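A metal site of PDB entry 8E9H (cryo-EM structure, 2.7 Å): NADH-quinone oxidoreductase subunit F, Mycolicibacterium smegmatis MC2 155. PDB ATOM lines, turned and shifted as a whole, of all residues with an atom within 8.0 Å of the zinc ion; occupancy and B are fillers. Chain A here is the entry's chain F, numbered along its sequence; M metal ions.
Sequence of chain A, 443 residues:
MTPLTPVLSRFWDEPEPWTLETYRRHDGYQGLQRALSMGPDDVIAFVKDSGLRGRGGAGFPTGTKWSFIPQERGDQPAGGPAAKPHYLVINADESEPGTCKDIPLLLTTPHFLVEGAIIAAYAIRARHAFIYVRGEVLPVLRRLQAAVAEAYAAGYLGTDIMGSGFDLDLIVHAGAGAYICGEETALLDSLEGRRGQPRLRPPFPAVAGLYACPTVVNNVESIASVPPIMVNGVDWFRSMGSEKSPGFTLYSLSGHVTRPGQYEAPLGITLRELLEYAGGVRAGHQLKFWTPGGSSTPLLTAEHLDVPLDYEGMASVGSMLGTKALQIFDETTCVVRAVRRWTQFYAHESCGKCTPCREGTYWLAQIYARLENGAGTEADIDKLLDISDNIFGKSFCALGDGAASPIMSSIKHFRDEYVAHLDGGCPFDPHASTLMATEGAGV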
ATOM      1  N   THR A 333     -11.207   6.467 -24.556  1.00  0.00           N
ATOM      2  CA  THR A 333     -11.172   7.003 -25.913  1.00  0.00           C
ATOM      3  C   THR A 333     -12.131   8.169 -26.065  1.00  0.00           C
ATOM      4  O   THR A 333     -13.208   8.201 -25.459  1.00  0.00           O
ATOM      5  CB  THR A 333     -11.528   5.922 -26.920  1.00  0.00           C
ATOM      6  OG1 THR A 333     -12.884   5.504 -26.712  1.00  0.00           O
ATOM      7  CG2 THR A 333     -10.622   4.739 -26.760  1.00  0.00           C
ATOM      8  N   CYS A 334     -11.745   9.133 -26.887  1.00  0.00           N
ATOM      9  CA  CYS A 334     -12.600  10.257 -27.247  1.00  0.00           C
ATOM     10  C   CYS A 334     -13.232   9.974 -28.589  1.00  0.00           C
ATOM     11  O   CYS A 334     -12.531   9.852 -29.602  1.00  0.00           O
ATOM     12  CB  CYS A 334     -11.790  11.553 -27.303  1.00  0.00           C
ATOM     13  SG  CYS A 334     -12.693  12.983 -27.936  1.00  0.00           S
ATOM     14  N   VAL A 335     -14.567   9.882 -28.611  1.00  0.00           N
ATOM     15  CA  VAL A 335     -15.250   9.537 -29.851  1.00  0.00           C
ATOM     16  C   VAL A 335     -14.913  10.556 -30.930  1.00  0.00           C
ATOM     17  O   VAL A 335     -14.771  10.214 -32.110  1.00  0.00           O
ATOM     18  CB  VAL A 335     -16.768   9.442 -29.633  1.00  0.00           C
ATOM     19  CG1 VAL A 335     -17.073   8.480 -28.520  1.00  0.00           C
ATOM     20  CG2 VAL A 335     -17.347  10.817 -29.328  1.00  0.00           C
ATOM     21  N   VAL A 336     -14.769  11.826 -30.545  1.00  0.00           N
ATOM     22  CA  VAL A 336     -14.385  12.836 -31.525  1.00  0.00           C
ATOM     23  C   VAL A 336     -13.024  12.521 -32.107  1.00  0.00           C
ATOM     24  O   VAL A 336     -12.820  12.644 -33.315  1.00  0.00           O
ATOM     25  CB  VAL A 336     -14.422  14.237 -30.895  1.00  0.00           C
ATOM     26  CG1 VAL A 336     -14.126  15.283 -31.944  1.00  0.00           C
ATOM     27  CG2 VAL A 336     -15.775  14.486 -30.259  1.00  0.00           C
ATOM     28  N   ARG A 337     -12.055  12.113 -31.276  1.00  0.00           N
ATOM     29  CA  ARG A 337     -10.731  11.791 -31.790  1.00  0.00           C
ATOM     30  C   ARG A 337     -10.796  10.621 -32.761  1.00  0.00           C
ATOM     31  O   ARG A 337     -10.201  10.659 -33.849  1.00  0.00           O
ATOM     32  CB  ARG A 337      -9.789  11.474 -30.636  1.00  0.00           C
ATOM     33  CG  ARG A 337      -8.386  11.115 -31.092  1.00  0.00           C
ATOM     34  CD  ARG A 337      -7.365  11.355 -29.998  1.00  0.00           C
ATOM     35  NE  ARG A 337      -7.303  10.242 -29.068  1.00  0.00           N
ATOM     36  CZ  ARG A 337      -6.316   9.353 -29.002  1.00  0.00           C
ATOM     37  NH1 ARG A 337      -5.281   9.415 -29.819  1.00  0.00           N
ATOM     38  NH2 ARG A 337      -6.371   8.388 -28.100  1.00  0.00           N
ATOM     39  N   ALA A 338     -11.507   9.560 -32.387  1.00  0.00           N
ATOM     40  CA  ALA A 338     -11.580   8.385 -33.241  1.00  0.00           C
ATOM     41  C   ALA A 338     -12.250   8.715 -34.572  1.00  0.00           C
ATOM     42  O   ALA A 338     -11.778   8.316 -35.639  1.00  0.00           O
ATOM     43  CB  ALA A 338     -12.348   7.268 -32.523  1.00  0.00           C
ATOM     44  N   ARG A 340     -12.448  11.649 -35.944  1.00  0.00           N
ATOM     45  CA  ARG A 340     -11.554  12.506 -36.712  1.00  0.00           C
ATOM     46  C   ARG A 340     -10.513  11.683 -37.443  1.00  0.00           C
ATOM     47  O   ARG A 340     -10.201  11.946 -38.616  1.00  0.00           O
ATOM     48  CB  ARG A 340     -10.863  13.502 -35.795  1.00  0.00           C
ATOM     49  CG  ARG A 340      -9.881  14.384 -36.545  1.00  0.00           C
ATOM     50  CD  ARG A 340      -9.506  15.620 -35.778  1.00  0.00           C
ATOM     51  NE  ARG A 340      -8.212  15.486 -35.108  1.00  0.00           N
ATOM     52  CZ  ARG A 340      -7.064  15.924 -35.615  1.00  0.00           C
ATOM     53  NH1 ARG A 340      -6.999  16.523 -36.791  1.00  0.00           N
ATOM     54  NH2 ARG A 340      -5.953  15.767 -34.913  1.00  0.00           N
ATOM     55  N   TYR A 368     -13.301  18.511 -37.897  1.00  0.00           N
ATOM     56  CA  TYR A 368     -12.924  17.686 -36.758  1.00  0.00           C
ATOM     57  C   TYR A 368     -11.589  18.126 -36.183  1.00  0.00           C
ATOM     58  O   TYR A 368     -11.392  18.093 -34.961  1.00  0.00           O
ATOM     59  CB  TYR A 368     -12.895  16.217 -37.156  1.00  0.00           C
ATOM     60  CG  TYR A 368     -14.202  15.521 -36.935  1.00  0.00           C
ATOM     61  CD1 TYR A 368     -14.545  15.014 -35.696  1.00  0.00           C
ATOM     62  CD2 TYR A 368     -15.109  15.366 -37.965  1.00  0.00           C
ATOM     63  CE1 TYR A 368     -15.732  14.371 -35.486  1.00  0.00           C
ATOM     64  CE2 TYR A 368     -16.311  14.728 -37.770  1.00  0.00           C
ATOM     65  CZ  TYR A 368     -16.615  14.232 -36.528  1.00  0.00           C
ATOM     66  OH  TYR A 368     -17.811  13.588 -36.329  1.00  0.00           O
ATOM     67  N   LEU A 371     -12.424  20.908 -34.039  1.00  0.00           N
ATOM     68  CA  LEU A 371     -13.070  20.451 -32.806  1.00  0.00           C
ATOM     69  C   LEU A 371     -12.045  19.966 -31.804  1.00  0.00           C
ATOM     70  O   LEU A 371     -12.031  20.405 -30.651  1.00  0.00           O
ATOM     71  CB  LEU A 371     -14.072  19.346 -33.105  1.00  0.00           C
ATOM     72  CG  LEU A 371     -15.391  19.706 -33.785  1.00  0.00           C
ATOM     73  CD1 LEU A 371     -16.331  18.521 -33.743  1.00  0.00           C
ATOM     74  CD2 LEU A 371     -16.037  20.908 -33.126  1.00  0.00           C
ATOM     75  N   GLU A 372     -11.167  19.051 -32.220  1.00  0.00           N
ATOM     76  CA  GLU A 372     -10.215  18.473 -31.287  1.00  0.00           C
ATOM     77  C   GLU A 372      -9.262  19.519 -30.751  1.00  0.00           C
ATOM     78  O   GLU A 372      -8.804  19.429 -29.609  1.00  0.00           O
ATOM     79  CB  GLU A 372      -9.439  17.343 -31.966  1.00  0.00           C
ATOM     80  CG  GLU A 372     -10.202  16.037 -32.039  1.00  0.00           C
ATOM     81  CD  GLU A 372     -10.202  15.285 -30.718  1.00  0.00           C
ATOM     82  OE1 GLU A 372      -9.107  14.994 -30.201  1.00  0.00           O
ATOM     83  OE2 GLU A 372     -11.297  14.990 -30.205  1.00  0.00           O
ATOM     84  N   ASN A 373      -8.943  20.535 -31.561  1.00  0.00           N
ATOM     85  CA  ASN A 373      -8.009  21.574 -31.164  1.00  0.00           C
ATOM     86  C   ASN A 373      -8.663  22.672 -30.325  1.00  0.00           C
ATOM     87  O   ASN A 373      -7.962  23.610 -29.931  1.00  0.00           O
ATOM     88  CB  ASN A 373      -7.363  22.195 -32.394  1.00  0.00           C
ATOM     89  CG  ASN A 373      -6.569  21.188 -33.200  1.00  0.00           C
ATOM     90  OD1 ASN A 373      -6.318  20.071 -32.734  1.00  0.00           O
ATOM     91  ND2 ASN A 373      -6.177  21.562 -34.402  1.00  0.00           N
ATOM     92  N   GLU A 417     -20.677  14.466 -25.797  1.00  0.00           N
ATOM     93  CA  GLU A 417     -19.225  14.579 -25.871  1.00  0.00           C
ATOM     94  C   GLU A 417     -18.813  15.595 -26.930  1.00  0.00           C
ATOM     95  O   GLU A 417     -17.844  16.348 -26.736  1.00  0.00           O
ATOM     96  CB  GLU A 417     -18.609  13.208 -26.180  1.00  0.00           C
ATOM     97  N   HIS A 421     -16.528  18.938 -26.182  1.00  0.00           N
ATOM     98  CA  HIS A 421     -15.303  19.350 -26.858  1.00  0.00           C
ATOM     99  C   HIS A 421     -15.277  20.842 -27.164  1.00  0.00           C
ATOM    100  O   HIS A 421     -14.196  21.416 -27.290  1.00  0.00           O
ATOM    101  CB  HIS A 421     -15.127  18.567 -28.160  1.00  0.00           C
ATOM    102  CG  HIS A 421     -14.558  17.192 -27.956  1.00  0.00           C
ATOM    103  ND1 HIS A 421     -15.252  16.193 -27.318  1.00  0.00           N
ATOM    104  CD2 HIS A 421     -13.358  16.671 -28.296  1.00  0.00           C
ATOM    105  CE1 HIS A 421     -14.509  15.106 -27.282  1.00  0.00           C
ATOM    106  NE2 HIS A 421     -13.351  15.366 -27.870  1.00  0.00           N
ATOM    107  N   GLY A 425     -11.575  22.077 -26.328  1.00  0.00           N
ATOM    108  CA  GLY A 425     -10.990  21.002 -27.105  1.00  0.00           C
ATOM    109  C   GLY A 425     -11.205  19.654 -26.459  1.00  0.00           C
ATOM    110  O   GLY A 425     -12.101  19.453 -25.631  1.00  0.00           O
ATOM    111  N   CYS A 426     -10.348  18.718 -26.829  1.00  0.00           N
ATOM    112  CA  CYS A 426     -10.475  17.351 -26.317  1.00  0.00           C
ATOM    113  C   CYS A 426     -10.160  17.334 -24.818  1.00  0.00           C
ATOM    114  O   CYS A 426      -9.049  17.717 -24.422  1.00  0.00           O
ATOM    115  CB  CYS A 426      -9.523  16.427 -27.057  1.00  0.00           C
ATOM    116  SG  CYS A 426      -9.748  14.672 -26.648  1.00  0.00           S
ATOM    117  N   PRO A 427     -11.089  16.902 -23.969  1.00  0.00           N
ATOM    118  CA  PRO A 427     -10.772  16.770 -22.543  1.00  0.00           C
ATOM    119  C   PRO A 427     -10.063  15.482 -22.195  1.00  0.00           C
ATOM    120  O   PRO A 427      -9.341  15.442 -21.189  1.00  0.00           O
ATOM    121  CB  PRO A 427     -12.143  16.850 -21.867  1.00  0.00           C
ATOM    122  CG  PRO A 427     -13.066  16.275 -22.873  1.00  0.00           C
ATOM    123  CD  PRO A 427     -12.529  16.664 -24.221  1.00  0.00           C
ATOM    124  N   PHE A 428     -10.241  14.431 -22.994  1.00  0.00           N
ATOM    125  CA  PHE A 428      -9.639  13.138 -22.678  1.00  0.00           C
ATOM    126  C   PHE A 428      -8.132  13.183 -22.836  1.00  0.00           C
ATOM    127  O   PHE A 428      -7.612  13.842 -23.739  1.00  0.00           O
ATOM    128  CB  PHE A 428     -10.230  12.059 -23.586  1.00  0.00           C
ATOM    129  CG  PHE A 428     -11.710  11.883 -23.446  1.00  0.00           C
ATOM    130  CD1 PHE A 428     -12.579  12.741 -24.090  1.00  0.00           C
ATOM    131  CD2 PHE A 428     -12.232  10.864 -22.682  1.00  0.00           C
ATOM    132  CE1 PHE A 428     -13.936  12.577 -23.978  1.00  0.00           C
ATOM    133  CE2 PHE A 428     -13.596  10.697 -22.564  1.00  0.00           C
ATOM    134  CZ  PHE A 428     -14.444  11.555 -23.215  1.00  0.00           C
ATOM    135  N   ASP A 429      -7.436  12.496 -21.950  1.00  0.00           N
ATOM    136  CA  ASP A 429      -5.985  12.361 -22.073  1.00  0.00           C
ATOM    137  C   ASP A 429      -5.671  11.215 -23.025  1.00  0.00           C
ATOM    138  O   ASP A 429      -6.047  10.068 -22.741  1.00  0.00           O
ATOM    139  CB  ASP A 429      -5.355  12.104 -20.717  1.00  0.00           C
ATOM    140  N   PRO A 430      -5.000  11.453 -24.148  1.00  0.00           N
ATOM    141  CA  PRO A 430      -4.733  10.340 -25.074  1.00  0.00           C
ATOM    142  C   PRO A 430      -3.981   9.187 -24.444  1.00  0.00           C
ATOM    143  O   PRO A 430      -4.279   8.025 -24.725  1.00  0.00           O
ATOM    144  CB  PRO A 430      -3.918  11.004 -26.198  1.00  0.00           C
ATOM    145  CG  PRO A 430      -4.255  12.443 -26.113  1.00  0.00           C
ATOM    146  CD  PRO A 430      -4.471  12.726 -24.659  1.00  0.00           C
HETATM  147 ZN    ZN M   1     -11.231  14.691 -28.395  1.00  0.00          ZN
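N of Arg 337 lies close to OE2 of Glu 372.
O of Glu 417 lies within hydrogen-bond range of ND1 of His 421 (2.7 Å).
The backbone NH (N) of Phe 428 lies close to the side-chain sulfur (SG) of Cys 426, at 3.7 Å.
The side-chain sulfur (SG) of Cys 334 lies close to the backbone NH (N) of Arg 337 (3.5 Å).
The backbone NH (N) of Val 336 sits close to the side-chain sulfur (SG) of Cys 334.
Residues that only touch the zinc ion: Arg 337.
Within 4 Å of the zinc ion: Cys 334, Arg 337, Glu 372, His 421 and Cys 426.
The nearest printed residue that does not touch the zinc ion is Val 336 (4.1 Å).
The zinc ion is bound by OE2 of Glu 372 (1.8 Å), NE2 of His 421 (2.3 Å), SG of Cys 426 (2.3 Å) and SG of Cys 334 (2.3 Å).
The zinc ion has four donor atoms within binding distance.
Slightly farther from the zinc ion lies the side-chain carboxylate (OE1) of Glu 372 (2.8 Å).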
